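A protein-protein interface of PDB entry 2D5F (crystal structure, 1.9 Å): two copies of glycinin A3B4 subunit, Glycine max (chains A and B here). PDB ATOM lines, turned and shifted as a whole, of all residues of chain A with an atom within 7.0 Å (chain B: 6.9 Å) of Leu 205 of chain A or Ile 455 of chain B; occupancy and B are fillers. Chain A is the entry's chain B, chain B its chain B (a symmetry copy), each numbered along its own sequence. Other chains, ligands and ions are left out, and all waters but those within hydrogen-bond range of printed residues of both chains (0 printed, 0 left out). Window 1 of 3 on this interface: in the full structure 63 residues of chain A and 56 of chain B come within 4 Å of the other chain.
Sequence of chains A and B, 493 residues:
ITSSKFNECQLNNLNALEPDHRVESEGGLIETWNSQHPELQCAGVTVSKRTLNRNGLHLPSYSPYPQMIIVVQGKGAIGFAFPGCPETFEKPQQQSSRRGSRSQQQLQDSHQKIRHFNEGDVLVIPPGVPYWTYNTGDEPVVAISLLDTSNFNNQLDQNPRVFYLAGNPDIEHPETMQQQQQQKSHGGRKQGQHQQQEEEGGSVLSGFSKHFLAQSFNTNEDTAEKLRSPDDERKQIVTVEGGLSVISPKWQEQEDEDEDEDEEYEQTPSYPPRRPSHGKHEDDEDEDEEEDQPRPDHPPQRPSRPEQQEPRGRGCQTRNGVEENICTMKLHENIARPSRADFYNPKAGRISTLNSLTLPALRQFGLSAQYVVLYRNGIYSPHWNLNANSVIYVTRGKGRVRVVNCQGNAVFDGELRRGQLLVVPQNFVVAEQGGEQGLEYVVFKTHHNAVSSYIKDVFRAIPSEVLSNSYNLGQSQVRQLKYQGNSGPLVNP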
ATOM      1  N   TYR A  62     -15.374  11.142  -9.273  1.00  0.00           N
ATOM      2  CA  TYR A  62     -15.646  11.093 -10.706  1.00  0.00           C
ATOM      3  C   TYR A  62     -16.739  10.060 -10.987  1.00  0.00           C
ATOM      4  O   TYR A  62     -16.958   9.140 -10.193  1.00  0.00           O
ATOM      5  CB  TYR A  62     -14.382  10.752 -11.503  1.00  0.00           C
ATOM      6  CG  TYR A  62     -13.773   9.404 -11.189  1.00  0.00           C
ATOM      7  CD1 TYR A  62     -12.881   9.249 -10.128  1.00  0.00           C
ATOM      8  CD2 TYR A  62     -14.083   8.278 -11.958  1.00  0.00           C
ATOM      9  CE1 TYR A  62     -12.305   8.006  -9.842  1.00  0.00           C
ATOM     10  CE2 TYR A  62     -13.520   7.033 -11.679  1.00  0.00           C
ATOM     11  CZ  TYR A  62     -12.629   6.906 -10.618  1.00  0.00           C
ATOM     12  OH  TYR A  62     -12.070   5.682 -10.333  1.00  0.00           O
ATOM     13  N   TYR A 164     -15.393   7.906  -5.310  1.00  0.00           N
ATOM     14  CA  TYR A 164     -14.689   8.890  -4.497  1.00  0.00           C
ATOM     15  C   TYR A 164     -13.216   8.545  -4.372  1.00  0.00           C
ATOM     16  O   TYR A 164     -12.853   7.386  -4.167  1.00  0.00           O
ATOM     17  CB  TYR A 164     -15.313   9.018  -3.096  1.00  0.00           C
ATOM     18  CG  TYR A 164     -16.488   9.966  -3.051  1.00  0.00           C
ATOM     19  CD1 TYR A 164     -17.799   9.497  -3.155  1.00  0.00           C
ATOM     20  CD2 TYR A 164     -16.286  11.347  -2.974  1.00  0.00           C
ATOM     21  CE1 TYR A 164     -18.882  10.383  -3.188  1.00  0.00           C
ATOM     22  CE2 TYR A 164     -17.352  12.235  -3.009  1.00  0.00           C
ATOM     23  CZ  TYR A 164     -18.646  11.751  -3.118  1.00  0.00           C
ATOM     24  OH  TYR A 164     -19.692  12.640  -3.178  1.00  0.00           O
ATOM     25  N   LEU A 165     -12.371   9.557  -4.523  1.00  0.00           N
ATOM     26  CA  LEU A 165     -10.935   9.373  -4.405  1.00  0.00           C
ATOM     27  C   LEU A 165     -10.501   9.566  -2.953  1.00  0.00           C
ATOM     28  O   LEU A 165      -9.394   9.190  -2.570  1.00  0.00           O
ATOM     29  CB  LEU A 165     -10.206  10.375  -5.304  1.00  0.00           C
ATOM     30  CG  LEU A 165     -10.214  10.055  -6.801  1.00  0.00           C
ATOM     31  CD1 LEU A 165      -9.899  11.293  -7.603  1.00  0.00           C
ATOM     32  CD2 LEU A 165      -9.207   8.957  -7.078  1.00  0.00           C
ATOM     33  N   ALA A 166     -11.378  10.157  -2.148  1.00  0.00           N
ATOM     34  CA  ALA A 166     -11.068  10.406  -0.742  1.00  0.00           C
ATOM     35  C   ALA A 166     -12.301  10.352   0.144  1.00  0.00           C
ATOM     36  O   ALA A 166     -13.433  10.391  -0.337  1.00  0.00           O
ATOM     37  CB  ALA A 166     -10.389  11.768  -0.587  1.00  0.00           C
ATOM     38  N   GLY A 202     -17.397   3.696   0.406  1.00  0.00           N
ATOM     39  CA  GLY A 202     -15.965   3.685   0.645  1.00  0.00           C
ATOM     40  C   GLY A 202     -15.278   4.338  -0.544  1.00  0.00           C
ATOM     41  O   GLY A 202     -15.820   4.322  -1.648  1.00  0.00           O
ATOM     42  N   SER A 203     -14.102   4.921  -0.329  1.00  0.00           N
ATOM     43  CA  SER A 203     -13.364   5.553  -1.418  1.00  0.00           C
ATOM     44  C   SER A 203     -12.703   4.448  -2.234  1.00  0.00           C
ATOM     45  O   SER A 203     -12.634   3.306  -1.789  1.00  0.00           O
ATOM     46  CB  SER A 203     -12.296   6.493  -0.862  1.00  0.00           C
ATOM     47  OG  SER A 203     -11.295   5.757  -0.188  1.00  0.00           O
ATOM     48  N   VAL A 204     -12.222   4.772  -3.428  1.00  0.00           N
ATOM     49  CA  VAL A 204     -11.580   3.756  -4.244  1.00  0.00           C
ATOM     50  C   VAL A 204     -10.244   3.364  -3.630  1.00  0.00           C
ATOM     51  O   VAL A 204      -9.778   2.232  -3.789  1.00  0.00           O
ATOM     52  CB  VAL A 204     -11.376   4.243  -5.693  1.00  0.00           C
ATOM     53  CG1 VAL A 204     -12.734   4.493  -6.335  1.00  0.00           C
ATOM     54  CG2 VAL A 204     -10.532   5.503  -5.717  1.00  0.00           C
ATOM     55  N   LEU A 205      -9.645   4.298  -2.899  1.00  0.00           N
ATOM     56  CA  LEU A 205      -8.361   4.046  -2.257  1.00  0.00           C
ATOM     57  C   LEU A 205      -8.498   3.101  -1.062  1.00  0.00           C
ATOM     58  O   LEU A 205      -7.573   2.353  -0.751  1.00  0.00           O
ATOM     59  CB  LEU A 205      -7.726   5.375  -1.831  1.00  0.00           C
ATOM     60  CG  LEU A 205      -6.499   5.838  -2.629  1.00  0.00           C
ATOM     61  CD1 LEU A 205      -6.643   5.465  -4.084  1.00  0.00           C
ATOM     62  CD2 LEU A 205      -6.318   7.337  -2.470  1.00  0.00           C
ATOM     63  N   SER A 206      -9.657   3.116  -0.408  1.00  0.00           N
ATOM     64  CA  SER A 206      -9.876   2.239   0.741  1.00  0.00           C
ATOM     65  C   SER A 206      -9.958   0.775   0.306  1.00  0.00           C
ATOM     66  O   SER A 206      -9.995  -0.126   1.142  1.00  0.00           O
ATOM     67  CB  SER A 206     -11.158   2.630   1.486  1.00  0.00           C
ATOM     68  OG  SER A 206     -12.320   2.323   0.734  1.00  0.00           O
ATOM     69  N   GLY A 207      -9.976   0.547  -1.006  1.00  0.00           N
ATOM     70  CA  GLY A 207     -10.052  -0.807  -1.529  1.00  0.00           C
ATOM     71  C   GLY A 207      -8.688  -1.462  -1.669  1.00  0.00           C
ATOM     72  O   GLY A 207      -8.593  -2.646  -1.990  1.00  0.00           O
ATOM     73  N   PHE A 208      -7.637  -0.683  -1.432  1.00  0.00           N
ATOM     74  CA  PHE A 208      -6.262  -1.165  -1.517  1.00  0.00           C
ATOM     75  C   PHE A 208      -5.655  -1.187  -0.112  1.00  0.00           C
ATOM     76  O   PHE A 208      -6.043  -0.398   0.748  1.00  0.00           O
ATOM     77  CB  PHE A 208      -5.431  -0.234  -2.405  1.00  0.00           C
ATOM     78  CG  PHE A 208      -5.847  -0.236  -3.849  1.00  0.00           C
ATOM     79  CD1 PHE A 208      -5.359  -1.202  -4.725  1.00  0.00           C
ATOM     80  CD2 PHE A 208      -6.733   0.728  -4.333  1.00  0.00           C
ATOM     81  CE1 PHE A 208      -5.744  -1.212  -6.063  1.00  0.00           C
ATOM     82  CE2 PHE A 208      -7.126   0.730  -5.666  1.00  0.00           C
ATOM     83  CZ  PHE A 208      -6.631  -0.244  -6.535  1.00  0.00           C
ATOM     84  N   SER A 209      -4.700  -2.084   0.113  1.00  0.00           N
ATOM     85  CA  SER A 209      -4.043  -2.189   1.415  1.00  0.00           C
ATOM     86  C   SER A 209      -3.050  -1.045   1.574  1.00  0.00           C
ATOM     87  O   SER A 209      -2.472  -0.585   0.586  1.00  0.00           O
ATOM     88  CB  SER A 209      -3.292  -3.515   1.519  1.00  0.00           C
ATOM     89  OG  SER A 209      -2.170  -3.514   0.652  1.00  0.00           O
ATOM     90  N   LYS A 210      -2.835  -0.589   2.808  1.00  0.00           N
ATOM     91  CA  LYS A 210      -1.893   0.505   3.035  1.00  0.00           C
ATOM     92  C   LYS A 210      -0.496   0.129   2.565  1.00  0.00           C
ATOM     93  O   LYS A 210       0.263   0.977   2.102  1.00  0.00           O
ATOM     94  CB  LYS A 210      -1.844   0.908   4.517  1.00  0.00           C
ATOM     95  CG  LYS A 210      -1.320  -0.158   5.474  1.00  0.00           C
ATOM     96  CD  LYS A 210      -1.234   0.391   6.907  1.00  0.00           C
ATOM     97  CE  LYS A 210      -1.084  -0.726   7.932  1.00  0.00           C
ATOM     98  NZ  LYS A 210       0.034  -1.640   7.572  1.00  0.00           N
ATOM     99  N   LEU A 213      -0.423   0.675  -1.181  1.00  0.00           N
ATOM    100  CA  LEU A 213      -0.505   2.094  -1.493  1.00  0.00           C
ATOM    101  C   LEU A 213       0.838   2.713  -1.143  1.00  0.00           C
ATOM    102  O   LEU A 213       1.341   3.579  -1.862  1.00  0.00           O
ATOM    103  CB  LEU A 213      -1.622   2.774  -0.693  1.00  0.00           C
ATOM    104  CG  LEU A 213      -3.059   2.397  -1.086  1.00  0.00           C
ATOM    105  CD1 LEU A 213      -4.048   3.249  -0.300  1.00  0.00           C
ATOM    106  CD2 LEU A 213      -3.263   2.605  -2.592  1.00  0.00           C
ATOM    107  N   PHE A 217       2.667   4.569  -4.196  1.00  0.00           N
ATOM    108  CA  PHE A 217       2.899   6.002  -4.114  1.00  0.00           C
ATOM    109  C   PHE A 217       4.249   6.396  -3.512  1.00  0.00           C
ATOM    110  O   PHE A 217       4.499   7.577  -3.269  1.00  0.00           O
ATOM    111  CB  PHE A 217       1.761   6.645  -3.311  1.00  0.00           C
ATOM    112  CG  PHE A 217       0.391   6.411  -3.901  1.00  0.00           C
ATOM    113  CD1 PHE A 217      -0.732   6.348  -3.078  1.00  0.00           C
ATOM    114  CD2 PHE A 217       0.223   6.260  -5.280  1.00  0.00           C
ATOM    115  CE1 PHE A 217      -1.999   6.135  -3.611  1.00  0.00           C
ATOM    116  CE2 PHE A 217      -1.046   6.047  -5.828  1.00  0.00           C
ATOM    117  CZ  PHE A 217      -2.159   5.984  -4.990  1.00  0.00           C
ATOM    118  N   ALA A 224      -0.021   6.289   3.805  1.00  0.00           N
ATOM    119  CA  ALA A 224      -0.858   5.386   3.024  1.00  0.00           C
ATOM    120  C   ALA A 224      -2.135   4.985   3.757  1.00  0.00           C
ATOM    121  O   ALA A 224      -3.191   4.853   3.136  1.00  0.00           O
ATOM    122  CB  ALA A 224      -0.066   4.143   2.629  1.00  0.00           C
ATOM    123  N   LEU A 227      -4.603   7.640   3.543  1.00  0.00           N
ATOM    124  CA  LEU A 227      -5.142   7.731   2.191  1.00  0.00           C
ATOM    125  C   LEU A 227      -6.375   6.854   2.039  1.00  0.00           C
ATOM    126  O   LEU A 227      -7.156   7.029   1.106  1.00  0.00           O
ATOM    127  CB  LEU A 227      -4.088   7.311   1.164  1.00  0.00           C
ATOM    128  CG  LEU A 227      -2.959   8.311   0.918  1.00  0.00           C
ATOM    129  CD1 LEU A 227      -2.030   7.767  -0.162  1.00  0.00           C
ATOM    130  CD2 LEU A 227      -3.537   9.654   0.490  1.00  0.00           C
ATOM    131  N   ARG A 228      -6.549   5.919   2.971  1.00  0.00           N
ATOM    132  CA  ARG A 228      -7.684   5.004   2.951  1.00  0.00           C
ATOM    133  C   ARG A 228      -8.865   5.522   3.777  1.00  0.00           C
ATOM    134  O   ARG A 228      -9.921   4.897   3.810  1.00  0.00           O
ATOM    135  CB  ARG A 228      -7.252   3.625   3.470  1.00  0.00           C
ATOM    136  CG  ARG A 228      -6.057   3.040   2.729  1.00  0.00           C
ATOM    137  CD  ARG A 228      -5.602   1.700   3.303  1.00  0.00           C
ATOM    138  NE  ARG A 228      -6.562   0.629   3.053  1.00  0.00           N
ATOM    139  CZ  ARG A 228      -7.307   0.052   3.988  1.00  0.00           C
ATOM    140  NH1 ARG A 228      -8.156  -0.913   3.659  1.00  0.00           N
ATOM    141  NH2 ARG A 228      -7.204   0.434   5.254  1.00  0.00           N
ATOM    142  N   SER A 229      -8.683   6.666   4.431  1.00  0.00           N
ATOM    143  CA  SER A 229      -9.733   7.272   5.257  1.00  0.00           C
ATOM    144  C   SER A 229     -10.350   6.268   6.233  1.00  0.00           C
ATOM    145  O   SER A 229     -11.571   6.156   6.326  1.00  0.00           O
ATOM    146  CB  SER A 229     -10.839   7.840   4.365  1.00  0.00           C
ATOM    147  OG  SER A 229     -10.309   8.717   3.394  1.00  0.00           O
ATOM    148  N   SER B 381       0.897   1.530 -10.865  1.00  0.00           N
ATOM    149  CA  SER B 381       0.078   2.127  -9.811  1.00  0.00           C
ATOM    150  C   SER B 381      -1.405   2.291 -10.138  1.00  0.00           C
ATOM    151  O   SER B 381      -1.796   2.324 -11.304  1.00  0.00           O
ATOM    152  CB  SER B 381       0.680   3.473  -9.387  1.00  0.00           C
ATOM    153  OG  SER B 381       0.884   4.324 -10.495  1.00  0.00           O
ATOM    154  N   PRO B 382      -2.253   2.388  -9.096  1.00  0.00           N
ATOM    155  CA  PRO B 382      -3.700   2.546  -9.257  1.00  0.00           C
ATOM    156  C   PRO B 382      -4.083   3.561 -10.329  1.00  0.00           C
ATOM    157  O   PRO B 382      -3.716   4.735 -10.264  1.00  0.00           O
ATOM    158  CB  PRO B 382      -4.153   2.960  -7.859  1.00  0.00           C
ATOM    159  CG  PRO B 382      -3.227   2.168  -6.988  1.00  0.00           C
ATOM    160  CD  PRO B 382      -1.891   2.375  -7.667  1.00  0.00           C
ATOM    161  N   HIS B 383      -4.826   3.082 -11.323  1.00  0.00           N
ATOM    162  CA  HIS B 383      -5.282   3.906 -12.432  1.00  0.00           C
ATOM    163  C   HIS B 383      -6.647   3.395 -12.875  1.00  0.00           C
ATOM    164  O   HIS B 383      -7.071   2.314 -12.464  1.00  0.00           O
ATOM    165  CB  HIS B 383      -4.295   3.803 -13.604  1.00  0.00           C
ATOM    166  CG  HIS B 383      -4.086   2.404 -14.105  1.00  0.00           C
ATOM    167  ND1 HIS B 383      -3.324   1.473 -13.430  1.00  0.00           N
ATOM    168  CD2 HIS B 383      -4.535   1.780 -15.223  1.00  0.00           C
ATOM    169  CE1 HIS B 383      -3.309   0.340 -14.110  1.00  0.00           C
ATOM    170  NE2 HIS B 383      -4.037   0.498 -15.201  1.00  0.00           N
ATOM    171  N   TRP B 384      -7.338   4.181 -13.694  1.00  0.00           N
ATOM    172  CA  TRP B 384      -8.636   3.776 -14.224  1.00  0.00           C
ATOM    173  C   TRP B 384      -8.817   4.333 -15.629  1.00  0.00           C
ATOM    174  O   TRP B 384      -8.103   5.245 -16.050  1.00  0.00           O
ATOM    175  CB  TRP B 384      -9.771   4.256 -13.315  1.00  0.00           C
ATOM    176  CG  TRP B 384     -10.093   5.718 -13.436  1.00  0.00           C
ATOM    177  CD1 TRP B 384     -10.976   6.295 -14.303  1.00  0.00           C
ATOM    178  CD2 TRP B 384      -9.539   6.786 -12.659  1.00  0.00           C
ATOM    179  NE1 TRP B 384     -11.010   7.655 -14.109  1.00  0.00           N
ATOM    180  CE2 TRP B 384     -10.136   7.982 -13.108  1.00  0.00           C
ATOM    181  CE3 TRP B 384      -8.594   6.846 -11.628  1.00  0.00           C
ATOM    182  CZ2 TRP B 384      -9.820   9.232 -12.559  1.00  0.00           C
ATOM    183  CZ3 TRP B 384      -8.277   8.087 -11.084  1.00  0.00           C
ATOM    184  CH2 TRP B 384      -8.890   9.262 -11.551  1.00  0.00           C
ATOM    185  N   VAL B 404     -10.870  -2.406  -7.936  1.00  0.00           N
ATOM    186  CA  VAL B 404     -11.742  -1.830  -6.918  1.00  0.00           C
ATOM    187  C   VAL B 404     -12.896  -1.059  -7.562  1.00  0.00           C
ATOM    188  O   VAL B 404     -12.667  -0.285  -8.490  1.00  0.00           O
ATOM    189  CB  VAL B 404     -10.936  -0.864  -6.015  1.00  0.00           C
ATOM    190  CG1 VAL B 404     -11.846  -0.192  -4.997  1.00  0.00           C
ATOM    191  CG2 VAL B 404      -9.820  -1.628  -5.322  1.00  0.00           C
ATOM    192  N   ASN B 405     -14.124  -1.270  -7.078  1.00  0.00           N
ATOM    193  CA  ASN B 405     -15.295  -0.580  -7.633  1.00  0.00           C
ATOM    194  C   ASN B 405     -15.638   0.732  -6.920  1.00  0.00           C
ATOM    195  O   ASN B 405     -14.864   1.210  -6.085  1.00  0.00           O
ATOM    196  CB  ASN B 405     -16.521  -1.498  -7.631  1.00  0.00           C
ATOM    197  CG  ASN B 405     -17.022  -1.821  -6.234  1.00  0.00           C
ATOM    198  OD1 ASN B 405     -16.638  -1.185  -5.252  1.00  0.00           O
ATOM    199  ND2 ASN B 405     -17.900  -2.814  -6.144  1.00  0.00           N
ATOM    200  N   GLY B 408     -15.479   1.020  -3.039  1.00  0.00           N
ATOM    201  CA  GLY B 408     -14.206   0.762  -2.389  1.00  0.00           C
ATOM    202  C   GLY B 408     -13.945  -0.708  -2.117  1.00  0.00           C
ATOM    203  O   GLY B 408     -13.132  -1.058  -1.263  1.00  0.00           O
ATOM    204  N   VAL B 429     -11.027   1.112 -10.532  1.00  0.00           N
ATOM    205  CA  VAL B 429      -9.607   1.341 -10.334  1.00  0.00           C
ATOM    206  C   VAL B 429      -8.841   0.025 -10.298  1.00  0.00           C
ATOM    207  O   VAL B 429      -9.230  -0.915  -9.601  1.00  0.00           O
ATOM    208  CB  VAL B 429      -9.379   2.133  -9.043  1.00  0.00           C
ATOM    209  CG1 VAL B 429      -7.889   2.413  -8.850  1.00  0.00           C
ATOM    210  CG2 VAL B 429     -10.179   3.437  -9.108  1.00  0.00           C
ATOM    211  N   SER B 453      -6.184   7.428 -16.350  1.00  0.00           N
ATOM    212  CA  SER B 453      -5.603   8.375 -15.422  1.00  0.00           C
ATOM    213  C   SER B 453      -5.030   7.565 -14.271  1.00  0.00           C
ATOM    214  O   SER B 453      -5.619   6.562 -13.874  1.00  0.00           O
ATOM    215  CB  SER B 453      -6.679   9.334 -14.907  1.00  0.00           C
ATOM    216  OG  SER B 453      -6.150  10.206 -13.922  1.00  0.00           O
ATOM    217  N   TYR B 454      -3.867   7.961 -13.764  1.00  0.00           N
ATOM    218  CA  TYR B 454      -3.293   7.253 -12.625  1.00  0.00           C
ATOM    219  C   TYR B 454      -3.346   8.196 -11.416  1.00  0.00           C
ATOM    220  O   TYR B 454      -3.143   9.406 -11.544  1.00  0.00           O
ATOM    221  CB  TYR B 454      -1.877   6.743 -12.930  1.00  0.00           C
ATOM    222  CG  TYR B 454      -0.828   7.766 -13.314  1.00  0.00           C
ATOM    223  CD1 TYR B 454       0.246   8.040 -12.459  1.00  0.00           C
ATOM    224  CD2 TYR B 454      -0.855   8.396 -14.558  1.00  0.00           C
ATOM    225  CE1 TYR B 454       1.269   8.906 -12.834  1.00  0.00           C
ATOM    226  CE2 TYR B 454       0.166   9.268 -14.946  1.00  0.00           C
ATOM    227  CZ  TYR B 454       1.225   9.516 -14.080  1.00  0.00           C
ATOM    228  OH  TYR B 454       2.238  10.370 -14.461  1.00  0.00           O
ATOM    229  N   ILE B 455      -3.663   7.646 -10.251  1.00  0.00           N
ATOM    230  CA  ILE B 455      -3.821   8.465  -9.063  1.00  0.00           C
ATOM    231  C   ILE B 455      -2.627   9.327  -8.655  1.00  0.00           C
ATOM    232  O   ILE B 455      -2.818  10.427  -8.146  1.00  0.00           O
ATOM    233  CB  ILE B 455      -4.331   7.601  -7.890  1.00  0.00           C
ATOM    234  CG1 ILE B 455      -5.714   7.052  -8.270  1.00  0.00           C
ATOM    235  CG2 ILE B 455      -4.416   8.430  -6.599  1.00  0.00           C
ATOM    236  CD1 ILE B 455      -6.372   6.135  -7.259  1.00  0.00           C
ATOM    237  N   LYS B 456      -1.405   8.862  -8.879  1.00  0.00           N
ATOM    238  CA  LYS B 456      -0.243   9.689  -8.532  1.00  0.00           C
ATOM    239  C   LYS B 456      -0.367  11.038  -9.252  1.00  0.00           C
ATOM    240  O   LYS B 456      -0.186  12.099  -8.655  1.00  0.00           O
ATOM    241  CB  LYS B 456       1.064   9.016  -8.962  1.00  0.00           C
ATOM    242  CG  LYS B 456       1.408   7.750  -8.205  1.00  0.00           C
ATOM    243  CD  LYS B 456       2.692   7.120  -8.739  1.00  0.00           C
ATOM    244  CE  LYS B 456       3.872   8.086  -8.623  1.00  0.00           C
ATOM    245  NZ  LYS B 456       5.103   7.547  -9.265  1.00  0.00           N
ATOM    246  N   ASP B 457      -0.684  10.985 -10.541  1.00  0.00           N
ATOM    247  CA  ASP B 457      -0.832  12.187 -11.348  1.00  0.00           C
ATOM    248  C   ASP B 457      -2.001  13.039 -10.857  1.00  0.00           C
ATOM    249  O   ASP B 457      -1.983  14.266 -10.977  1.00  0.00           O
ATOM    250  CB  ASP B 457      -1.032  11.799 -12.815  1.00  0.00           C
ATOM    251  CG  ASP B 457      -1.211  13.001 -13.721  1.00  0.00           C
ATOM    252  OD1 ASP B 457      -0.261  13.800 -13.863  1.00  0.00           O
ATOM    253  OD2 ASP B 457      -2.310  13.147 -14.290  1.00  0.00           O
ATOM    254  N   VAL B 458      -3.020  12.386 -10.309  1.00  0.00           N
ATOM    255  CA  VAL B 458      -4.186  13.099  -9.795  1.00  0.00           C
ATOM    256  C   VAL B 458      -3.781  13.938  -8.586  1.00  0.00           C
ATOM    257  O   VAL B 458      -4.193  15.091  -8.458  1.00  0.00           O
ATOM    258  CB  VAL B 458      -5.314  12.120  -9.380  1.00  0.00           C
ATOM    259  CG1 VAL B 458      -6.452  12.887  -8.732  1.00  0.00           C
ATOM    260  CG2 VAL B 458      -5.826  11.368 -10.604  1.00  0.00           C
ATOM    261  N   PHE B 459      -2.969  13.363  -7.701  1.00  0.00           N
ATOM    262  CA  PHE B 459      -2.511  14.099  -6.520  1.00  0.00           C
ATOM    263  C   PHE B 459      -1.800  15.382  -6.956  1.00  0.00           C
ATOM    264  O   PHE B 459      -1.981  16.440  -6.353  1.00  0.00           O
ATOM    265  CB  PHE B 459      -1.537  13.248  -5.690  1.00  0.00           C
ATOM    266  CG  PHE B 459      -2.180  12.082  -4.987  1.00  0.00           C
ATOM    267  CD1 PHE B 459      -1.446  10.925  -4.734  1.00  0.00           C
ATOM    268  CD2 PHE B 459      -3.505  12.136  -4.574  1.00  0.00           C
ATOM    269  CE1 PHE B 459      -2.025   9.836  -4.080  1.00  0.00           C
ATOM    270  CE2 PHE B 459      -4.096  11.050  -3.917  1.00  0.00           C
ATOM    271  CZ  PHE B 459      -3.354   9.901  -3.672  1.00  0.00           C
ATOM    272  N   ARG B 460      -1.002  15.285  -8.015  1.00  0.00           N
ATOM    273  CA  ARG B 460      -0.260  16.440  -8.505  1.00  0.00           C
ATOM    274  C   ARG B 460      -1.155  17.559  -9.025  1.00  0.00           C
ATOM    275  O   ARG B 460      -0.788  18.734  -8.965  1.00  0.00           O
ATOM    276  CB  ARG B 460       0.721  16.015  -9.603  1.00  0.00           C
ATOM    277  CG  ARG B 460       1.775  15.015  -9.143  1.00  0.00           C
ATOM    278  CD  ARG B 460       2.983  15.016 -10.062  1.00  0.00           C
ATOM    279  NE  ARG B 460       2.694  14.478 -11.388  1.00  0.00           N
ATOM    280  CZ  ARG B 460       2.687  13.182 -11.686  1.00  0.00           C
ATOM    281  NH1 ARG B 460       2.952  12.271 -10.754  1.00  0.00           N
ATOM    282  NH2 ARG B 460       2.429  12.794 -12.927  1.00  0.00           N
ATOM    283  N   TYR B 471      -7.601  13.933   3.131  1.00  0.00           N
ATOM    284  CA  TYR B 471      -7.029  12.771   3.804  1.00  0.00           C
ATOM    285  C   TYR B 471      -6.491  13.040   5.208  1.00  0.00           C
ATOM    286  O   TYR B 471      -5.890  12.157   5.824  1.00  0.00           O
ATOM    287  CB  TYR B 471      -5.895  12.184   2.956  1.00  0.00           C
ATOM    288  CG  TYR B 471      -6.281  11.844   1.532  1.00  0.00           C
ATOM    289  CD1 TYR B 471      -5.935  12.684   0.470  1.00  0.00           C
ATOM    290  CD2 TYR B 471      -6.986  10.675   1.243  1.00  0.00           C
ATOM    291  CE1 TYR B 471      -6.283  12.364  -0.850  1.00  0.00           C
ATOM    292  CE2 TYR B 471      -7.338  10.347  -0.067  1.00  0.00           C
ATOM    293  CZ  TYR B 471      -6.986  11.195  -1.111  1.00  0.00           C
ATOM    294  OH  TYR B 471      -7.333  10.866  -2.409  1.00  0.00           O
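O of Leu 165 of chain A lies within hydrogen-bond range of OH of Tyr 471 of chain B (2.7 Å).
The backbone carbonyl oxygen of Phe 208 of chain A sits at hydrogen-bond distance from the guanidinium group of Arg 228 of chain A (2.6 Å). The backbone carbonyl oxygen (O) of Pro 382 of chain B is in hydrogen-bond range of the backbone NH (N) of Ile 455 of chain B, at 2.9 Å. The backbone carbonyl oxygen of Tyr 164 of chain A is in hydrogen-bond range of the backbone NH of Val 204 of chain A (2.8 Å).
Among the printed residues, pairs that only touch across the chains: Ser 203 of chain A with Gly 408 of chain B (3.1 Å), Gly 207 of chain A with Gly 408 of chain B (3.1 Å), Tyr 62 of chain A with Val 429 of chain B (3.2 Å), Leu 205 of chain A with Ile 455 of chain B (3.3 Å), Ala 166 of chain A with Tyr 471 of chain B (3.4 Å), Val 204 of chain A with Val 404 of chain B (3.4 Å), Phe 217 of chain A with Lys 456 of chain B (3.5 Å), Leu 227 of chain A with Tyr 471 of chain B (3.5 Å), Tyr 62 of chain A with Trp 384 of chain B (3.5 Å), Phe 208 of chain A with Val 404 of chain B (3.6 Å), Gly 202 of chain A with Gly 408 of chain B (3.6 Å), Leu 205 of chain A with Tyr 471 of chain B (3.7 Å), Phe 208 of chain A with Val 429 of chain B (3.7 Å), Gly 207 of chain A with Val 404 of chain B (3.7 Å), Phe 217 of chain A with Ile 455 of chain B (3.7 Å), Val 204 of chain A with Val 429 of chain B (3.7 Å), Phe 217 of chain A with Phe 459 of chain B (3.7 Å), Val 204 of chain A with Asn 405 of chain B (3.9 Å), Leu 165 of chain A with Val 458 of chain B (3.96 Å) and Ser 206 of chain A with Gly 408 of chain B (3.97 Å).
Of chain B, only Ile 455 (3.3 Å) and Tyr 471 (3.7 Å) come within 4 Å of Leu 205 of chain A. Printed residues of chain A within 4 Å of Ile 455 of chain B: Leu 205 and Phe 217. Printed residues of chain A within 4 Å of Lys 456 of chain B: Phe 217 (3.5 Å). Printed residues of chain B within 4 Å of Gly 207 of chain A: Val 404 (3.7 Å) and Gly 408 (3.1 Å). Of the printed residues of chain B, Ser 206 of chain A touches Gly 408. Of the printed residues of chain B, Phe 217 of chain A touches Ile 455, Lys 456 and Phe 459. Of the printed residues of chain B, Gly 202 of chain A touches Gly 408. The nearest printed residue of chain A that does not touch Ile 455 of chain B is Leu 165 of chain A (4.004 Å).
Hydrophobic or aromatic side chains of chain A within 4 Å of the printed part of chain B: Tyr 62, Leu 165, Ala 166, Val 204, Leu 205, Phe 208, Phe 217 and Leu 227. Printed residues of chain B that touch a printed residue of chain A: Trp 384, Val 404, Asn 405, Gly 408, Val 429, Ile 455, Lys 456, Val 458, Phe 459 and Tyr 471. Hydrophobic or aromatic side chains of chain B within 4 Å of the printed part of chain A: Trp 384, Val 404, Val 429, Ile 455, Val 458, Phe 459 and Tyr 471. Among the printed residues, 21 pairs touch across the chains. Among the printed residues, no Asp or Glu carboxylate lies within 4 Å of a Lys or Arg side-chain nitrogen of the other chain.
No position is printed for both chains. Of the 21 pairs that touch across the chains among the printed residues, none has its exchanged pair printed and touching as well.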
